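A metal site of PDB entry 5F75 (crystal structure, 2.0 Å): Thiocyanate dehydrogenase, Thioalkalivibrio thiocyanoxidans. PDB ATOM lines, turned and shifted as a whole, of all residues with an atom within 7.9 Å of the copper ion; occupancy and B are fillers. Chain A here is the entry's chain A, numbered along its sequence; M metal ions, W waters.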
ATOM      1  N   LYS A 103      20.476  25.756 -12.055  1.00  0.00           N
ATOM      2  CA  LYS A 103      19.624  26.691 -12.825  1.00  0.00           C
ATOM      3  C   LYS A 103      18.349  27.011 -12.028  1.00  0.00           C
ATOM      4  O   LYS A 103      18.479  27.549 -10.918  1.00  0.00           O
ATOM      5  CB  LYS A 103      19.306  26.094 -14.197  1.00  0.00           C
ATOM      6  CG  LYS A 103      18.748  27.048 -15.223  1.00  0.00           C
ATOM      7  CD  LYS A 103      19.848  27.758 -15.972  1.00  0.00           C
ATOM      8  CE  LYS A 103      19.222  28.811 -16.875  1.00  0.00           C
ATOM      9  NZ  LYS A 103      20.162  29.395 -17.855  1.00  0.00           N
ATOM     10  N   ILE A 133      19.223  31.785 -10.063  1.00  0.00           N
ATOM     11  CA  ILE A 133      19.357  30.946 -11.260  1.00  0.00           C
ATOM     12  C   ILE A 133      20.841  30.598 -11.343  1.00  0.00           C
ATOM     13  O   ILE A 133      21.651  31.291 -11.977  1.00  0.00           O
ATOM     14  CB  ILE A 133      18.783  31.628 -12.559  1.00  0.00           C
ATOM     15  CG1 ILE A 133      17.267  31.886 -12.433  1.00  0.00           C
ATOM     16  CG2 ILE A 133      19.075  30.745 -13.805  1.00  0.00           C
ATOM     17  CD1 ILE A 133      16.703  32.828 -13.525  1.00  0.00           C
ATOM     18  N   MET A 134      21.211  29.527 -10.654  1.00  0.00           N
ATOM     19  CA  MET A 134      22.597  29.127 -10.523  1.00  0.00           C
ATOM     20  C   MET A 134      23.032  28.608 -11.906  1.00  0.00           C
ATOM     21  O   MET A 134      22.456  27.635 -12.432  1.00  0.00           O
ATOM     22  CB  MET A 134      22.728  28.042  -9.432  1.00  0.00           C
ATOM     23  CG  MET A 134      22.030  28.428  -8.124  1.00  0.00           C
ATOM     24  SD  MET A 134      22.935  29.799  -7.370  1.00  0.00           S
ATOM     25  CE  MET A 134      24.227  28.761  -6.641  1.00  0.00           C
ATOM     26  N   HIS A 135      24.055  29.250 -12.492  1.00  0.00           N
ATOM     27  CA  HIS A 135      24.291  29.126 -13.915  1.00  0.00           C
ATOM     28  C   HIS A 135      25.552  28.386 -14.328  1.00  0.00           C
ATOM     29  O   HIS A 135      25.552  27.140 -14.448  1.00  0.00           O
ATOM     30  CB  HIS A 135      24.173  30.502 -14.604  1.00  0.00           C
ATOM     31  CG  HIS A 135      23.845  30.383 -16.058  1.00  0.00           C
ATOM     32  ND1 HIS A 135      24.063  31.390 -16.964  1.00  0.00           N
ATOM     33  CD2 HIS A 135      23.356  29.336 -16.762  1.00  0.00           C
ATOM     34  CE1 HIS A 135      23.713  30.972 -18.179  1.00  0.00           C
ATOM     35  NE2 HIS A 135      23.284  29.736 -18.082  1.00  0.00           N
ATOM     36  N   HIS A 136      26.621  29.103 -14.585  1.00  0.00           N
ATOM     37  CA  HIS A 136      27.889  28.414 -14.882  1.00  0.00           C
ATOM     38  C   HIS A 136      28.853  28.301 -13.704  1.00  0.00           C
ATOM     39  O   HIS A 136      28.694  29.017 -12.692  1.00  0.00           O
ATOM     40  CB  HIS A 136      28.532  29.052 -16.097  1.00  0.00           C
ATOM     41  CG  HIS A 136      27.708  28.841 -17.334  1.00  0.00           C
ATOM     42  ND1 HIS A 136      27.641  27.624 -17.984  1.00  0.00           N
ATOM     43  CD2 HIS A 136      26.887  29.675 -18.027  1.00  0.00           C
ATOM     44  CE1 HIS A 136      26.816  27.726 -19.014  1.00  0.00           C
ATOM     45  NE2 HIS A 136      26.356  28.963 -19.070  1.00  0.00           N
ATOM     46  N   GLN A 156      21.990  34.175 -13.084  1.00  0.00           N
ATOM     47  CA  GLN A 156      21.253  35.117 -13.911  1.00  0.00           C
ATOM     48  C   GLN A 156      19.960  35.537 -13.263  1.00  0.00           C
ATOM     49  O   GLN A 156      19.433  34.847 -12.381  1.00  0.00           O
ATOM     50  CB  GLN A 156      20.895  34.498 -15.295  1.00  0.00           C
ATOM     51  CG  GLN A 156      22.101  34.203 -16.160  1.00  0.00           C
ATOM     52  CD  GLN A 156      21.732  33.436 -17.442  1.00  0.00           C
ATOM     53  OE1 GLN A 156      20.998  32.437 -17.417  1.00  0.00           O
ATOM     54  NE2 GLN A 156      22.298  33.870 -18.565  1.00  0.00           N
ATOM     55  N   ASN A 160      15.637  36.608 -17.589  1.00  0.00           N
ATOM     56  CA  ASN A 160      15.991  35.173 -17.749  1.00  0.00           C
ATOM     57  C   ASN A 160      15.057  34.238 -16.942  1.00  0.00           C
ATOM     58  O   ASN A 160      14.891  33.070 -17.278  1.00  0.00           O
ATOM     59  CB  ASN A 160      17.415  34.917 -17.345  1.00  0.00           C
ATOM     60  CG  ASN A 160      18.412  35.611 -18.249  1.00  0.00           C
ATOM     61  OD1 ASN A 160      18.632  35.190 -19.386  1.00  0.00           O
ATOM     62  ND2 ASN A 160      19.085  36.624 -17.717  1.00  0.00           N
ATOM     63  N   TYR A 164      11.703  29.957 -19.868  1.00  0.00           N
ATOM     64  CA  TYR A 164      11.594  28.458 -19.906  1.00  0.00           C
ATOM     65  C   TYR A 164      10.140  28.063 -19.679  1.00  0.00           C
ATOM     66  O   TYR A 164       9.313  28.934 -19.419  1.00  0.00           O
ATOM     67  CB  TYR A 164      12.549  27.775 -18.875  1.00  0.00           C
ATOM     68  CG  TYR A 164      14.011  28.120 -19.155  1.00  0.00           C
ATOM     69  CD1 TYR A 164      14.588  29.285 -18.616  1.00  0.00           C
ATOM     70  CD2 TYR A 164      14.790  27.338 -20.018  1.00  0.00           C
ATOM     71  CE1 TYR A 164      15.900  29.661 -18.918  1.00  0.00           C
ATOM     72  CE2 TYR A 164      16.117  27.699 -20.320  1.00  0.00           C
ATOM     73  CZ  TYR A 164      16.668  28.863 -19.771  1.00  0.00           C
ATOM     74  OH  TYR A 164      17.966  29.258 -20.044  1.00  0.00           O
ATOM     75  N   GLY A 204      27.045  37.002 -16.129  1.00  0.00           N
ATOM     76  CA  GLY A 204      26.087  35.906 -15.984  1.00  0.00           C
ATOM     77  C   GLY A 204      26.171  34.692 -16.899  1.00  0.00           C
ATOM     78  O   GLY A 204      25.263  33.823 -16.835  1.00  0.00           O
ATOM     79  N   VAL A 205      27.209  34.602 -17.742  1.00  0.00           N
ATOM     80  CA  VAL A 205      27.412  33.406 -18.610  1.00  0.00           C
ATOM     81  C   VAL A 205      28.664  32.621 -18.230  1.00  0.00           C
ATOM     82  O   VAL A 205      28.835  32.339 -17.043  1.00  0.00           O
ATOM     83  CB  VAL A 205      27.360  33.747 -20.127  1.00  0.00           C
ATOM     84  CG1 VAL A 205      27.119  32.479 -20.972  1.00  0.00           C
ATOM     85  CG2 VAL A 205      26.229  34.713 -20.359  1.00  0.00           C
ATOM     86  N   HIS A 206      29.544  32.265 -19.165  1.00  0.00           N
ATOM     87  CA  HIS A 206      30.500  31.181 -18.849  1.00  0.00           C
ATOM     88  C   HIS A 206      31.547  31.568 -17.856  1.00  0.00           C
ATOM     89  O   HIS A 206      32.058  32.690 -17.905  1.00  0.00           O
ATOM     90  CB  HIS A 206      31.142  30.523 -20.081  1.00  0.00           C
ATOM     91  CG  HIS A 206      30.175  29.705 -20.903  1.00  0.00           C
ATOM     92  ND1 HIS A 206      29.752  28.447 -20.523  1.00  0.00           N
ATOM     93  CD2 HIS A 206      29.482  30.009 -22.019  1.00  0.00           C
ATOM     94  CE1 HIS A 206      28.876  27.999 -21.392  1.00  0.00           C
ATOM     95  NE2 HIS A 206      28.703  28.910 -22.323  1.00  0.00           N
ATOM     96  N   GLU A 288      19.743  36.218 -21.893  1.00  0.00           N
ATOM     97  CA  GLU A 288      20.776  35.654 -22.741  1.00  0.00           C
ATOM     98  C   GLU A 288      20.063  34.910 -23.864  1.00  0.00           C
ATOM     99  O   GLU A 288      19.052  34.188 -23.615  1.00  0.00           O
ATOM    100  CB  GLU A 288      21.634  34.657 -21.938  1.00  0.00           C
ATOM    101  CG  GLU A 288      22.612  33.759 -22.694  1.00  0.00           C
ATOM    102  CD  GLU A 288      22.948  32.515 -21.867  1.00  0.00           C
ATOM    103  OE1 GLU A 288      22.445  32.385 -20.729  1.00  0.00           O
ATOM    104  OE2 GLU A 288      23.674  31.635 -22.343  1.00  0.00           O
ATOM    105  N   LEU A 289      20.610  35.033 -25.072  1.00  0.00           N
ATOM    106  CA  LEU A 289      20.034  34.375 -26.244  1.00  0.00           C
ATOM    107  C   LEU A 289      19.975  32.847 -26.002  1.00  0.00           C
ATOM    108  O   LEU A 289      20.987  32.233 -25.638  1.00  0.00           O
ATOM    109  CB  LEU A 289      20.934  34.650 -27.442  1.00  0.00           C
ATOM    110  CG  LEU A 289      20.959  36.116 -27.864  1.00  0.00           C
ATOM    111  CD1 LEU A 289      21.681  36.223 -29.198  1.00  0.00           C
ATOM    112  CD2 LEU A 289      19.558  36.742 -27.957  1.00  0.00           C
ATOM    113  N   PRO A 291      19.602  28.807 -27.369  1.00  0.00           N
ATOM    114  CA  PRO A 291      20.235  28.191 -28.554  1.00  0.00           C
ATOM    115  C   PRO A 291      19.332  28.454 -29.747  1.00  0.00           C
ATOM    116  O   PRO A 291      18.096  28.367 -29.617  1.00  0.00           O
ATOM    117  CB  PRO A 291      20.262  26.682 -28.206  1.00  0.00           C
ATOM    118  CG  PRO A 291      20.165  26.635 -26.707  1.00  0.00           C
ATOM    119  CD  PRO A 291      19.284  27.801 -26.338  1.00  0.00           C
ATOM    120  N   PHE A 436      26.595  22.826 -28.201  1.00  0.00           N
ATOM    121  CA  PHE A 436      27.131  23.996 -27.471  1.00  0.00           C
ATOM    122  C   PHE A 436      28.019  23.687 -26.263  1.00  0.00           C
ATOM    123  O   PHE A 436      28.430  24.605 -25.501  1.00  0.00           O
ATOM    124  CB  PHE A 436      26.030  25.050 -27.216  1.00  0.00           C
ATOM    125  CG  PHE A 436      24.918  24.589 -26.307  1.00  0.00           C
ATOM    126  CD1 PHE A 436      25.053  24.654 -24.900  1.00  0.00           C
ATOM    127  CD2 PHE A 436      23.727  24.152 -26.821  1.00  0.00           C
ATOM    128  CE1 PHE A 436      24.040  24.248 -24.041  1.00  0.00           C
ATOM    129  CE2 PHE A 436      22.699  23.737 -25.963  1.00  0.00           C
ATOM    130  CZ  PHE A 436      22.857  23.780 -24.583  1.00  0.00           C
ATOM    131  N   HIS A 437      28.354  22.415 -26.094  1.00  0.00           N
ATOM    132  CA  HIS A 437      29.322  22.012 -25.067  1.00  0.00           C
ATOM    133  C   HIS A 437      30.218  20.910 -25.561  1.00  0.00           C
ATOM    134  O   HIS A 437      29.820  20.143 -26.395  1.00  0.00           O
ATOM    135  CB  HIS A 437      28.621  21.520 -23.798  1.00  0.00           C
ATOM    136  CG  HIS A 437      27.760  22.546 -23.143  1.00  0.00           C
ATOM    137  ND1 HIS A 437      28.276  23.632 -22.464  1.00  0.00           N
ATOM    138  CD2 HIS A 437      26.408  22.659 -23.083  1.00  0.00           C
ATOM    139  CE1 HIS A 437      27.264  24.346 -21.978  1.00  0.00           C
ATOM    140  NE2 HIS A 437      26.129  23.789 -22.344  1.00  0.00           N
ATOM    141  N   HIS A 482      22.804  19.185 -21.595  1.00  0.00           N
ATOM    142  CA  HIS A 482      23.782  20.254 -21.370  1.00  0.00           C
ATOM    143  C   HIS A 482      25.264  19.868 -21.331  1.00  0.00           C
ATOM    144  O   HIS A 482      25.770  19.305 -22.283  1.00  0.00           O
ATOM    145  CB  HIS A 482      23.305  21.152 -20.232  1.00  0.00           C
ATOM    146  CG  HIS A 482      22.104  21.919 -20.619  1.00  0.00           C
ATOM    147  ND1 HIS A 482      22.170  23.118 -21.302  1.00  0.00           N
ATOM    148  CD2 HIS A 482      20.791  21.614 -20.514  1.00  0.00           C
ATOM    149  CE1 HIS A 482      20.943  23.550 -21.552  1.00  0.00           C
ATOM    150  NE2 HIS A 482      20.088  22.651 -21.087  1.00  0.00           N
ATOM    151  N   GLN A 501      14.124  22.565 -17.447  1.00  0.00           N
ATOM    152  CA  GLN A 501      13.686  23.086 -16.117  1.00  0.00           C
ATOM    153  C   GLN A 501      12.340  22.638 -15.641  1.00  0.00           C
ATOM    154  O   GLN A 501      11.917  23.076 -14.594  1.00  0.00           O
ATOM    155  CB  GLN A 501      13.657  24.624 -16.062  1.00  0.00           C
ATOM    156  CG  GLN A 501      14.906  25.296 -16.661  1.00  0.00           C
ATOM    157  CD  GLN A 501      16.189  24.844 -15.974  1.00  0.00           C
ATOM    158  OE1 GLN A 501      16.318  24.914 -14.741  1.00  0.00           O
ATOM    159  NE2 GLN A 501      17.148  24.378 -16.781  1.00  0.00           N
ATOM    160  N   GLY A 526      18.448  21.599 -12.855  1.00  0.00           N
ATOM    161  CA  GLY A 526      18.362  22.059 -14.252  1.00  0.00           C
ATOM    162  C   GLY A 526      19.714  22.416 -14.861  1.00  0.00           C
ATOM    163  O   GLY A 526      19.786  23.239 -15.787  1.00  0.00           O
ATOM    164  N   HIS A 527      20.766  21.807 -14.310  1.00  0.00           N
ATOM    165  CA  HIS A 527      22.170  22.016 -14.698  1.00  0.00           C
ATOM    166  C   HIS A 527      22.394  22.553 -16.093  1.00  0.00           C
ATOM    167  O   HIS A 527      22.059  21.867 -17.103  1.00  0.00           O
ATOM    168  CB  HIS A 527      23.020  20.721 -14.580  1.00  0.00           C
ATOM    169  CG  HIS A 527      22.296  19.551 -13.986  1.00  0.00           C
ATOM    170  ND1 HIS A 527      21.337  18.849 -14.679  1.00  0.00           N
ATOM    171  CD2 HIS A 527      22.411  18.958 -12.774  1.00  0.00           C
ATOM    172  CE1 HIS A 527      20.898  17.853 -13.918  1.00  0.00           C
ATOM    173  NE2 HIS A 527      21.528  17.904 -12.756  1.00  0.00           N
ATOM    174  N   HIS A 528      22.991  23.749 -16.162  1.00  0.00           N
ATOM    175  CA  HIS A 528      23.640  24.222 -17.409  1.00  0.00           C
ATOM    176  C   HIS A 528      25.154  24.159 -17.375  1.00  0.00           C
ATOM    177  O   HIS A 528      25.841  24.744 -18.222  1.00  0.00           O
ATOM    178  CB  HIS A 528      23.175  25.607 -17.817  1.00  0.00           C
ATOM    179  CG  HIS A 528      21.789  25.626 -18.370  1.00  0.00           C
ATOM    180  ND1 HIS A 528      21.278  26.678 -19.080  1.00  0.00           N
ATOM    181  CD2 HIS A 528      20.811  24.695 -18.322  1.00  0.00           C
ATOM    182  CE1 HIS A 528      20.025  26.421 -19.414  1.00  0.00           C
ATOM    183  NE2 HIS A 528      19.724  25.210 -18.993  1.00  0.00           N
ATOM    184  N   ASP A 529      25.690  23.448 -16.399  1.00  0.00           N
ATOM    185  CA  ASP A 529      27.146  23.265 -16.290  1.00  0.00           C
ATOM    186  C   ASP A 529      27.404  22.090 -15.348  1.00  0.00           C
ATOM    187  O   ASP A 529      26.524  21.703 -14.581  1.00  0.00           O
ATOM    188  CB  ASP A 529      27.824  24.551 -15.719  1.00  0.00           C
ATOM    189  CG  ASP A 529      29.081  24.898 -16.460  1.00  0.00           C
ATOM    190  OD1 ASP A 529      29.761  23.928 -16.822  1.00  0.00           O
ATOM    191  OD2 ASP A 529      29.373  26.109 -16.726  1.00  0.00           O
HETATM  192 CU    CU M   1      21.866  28.590 -18.991  1.00  0.00          CU
HETATM  193  O   HOH W   1      23.249  28.090 -20.032  1.00  0.00           O
HETATM  194  O   HOH W   2      21.534  29.846 -20.636  1.00  0.00           O
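The side-chain amino group (NZ) of Lys 103 sits close to the side-chain hydroxyl (OH) of Tyr 164.
NE2 of His 528 lies within hydrogen-bond range of NE2 of Gln 501 (3.5 Å).
The side-chain amino group of Lys 103 sits close to the side-chain amide oxygen of Gln 156.
The backbone carbonyl oxygen (O) of Gly 204 lies within hydrogen-bond range of a ring nitrogen (ND1) of His 135 (2.7 Å).
A ring nitrogen (ND1) of His 135 sits close to the side-chain amide oxygen (OE1) of Gln 156 (3.3 Å).
The backbone carbonyl oxygen of Met 134 sits at hydrogen-bond distance from the backbone NH of Lys 103 (2.8 Å).
A ring nitrogen (NE2) of His 135 lies close to a ring nitrogen (NE2) of His 136, at 3.3 Å.
A ring nitrogen (NE2) of His 528 sits close to a ring nitrogen (NE2) of His 482.
The nearest printed residue that does not touch the copper ion is Tyr 164 (4.1 Å).
The copper ion is bound by water W1, a ring nitrogen (ND1) of His 528, a ring nitrogen (NE2) of His 135, water W2 and the side-chain amino group (NZ) of Lys 103.
The copper ion has five donor atoms within binding distance.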
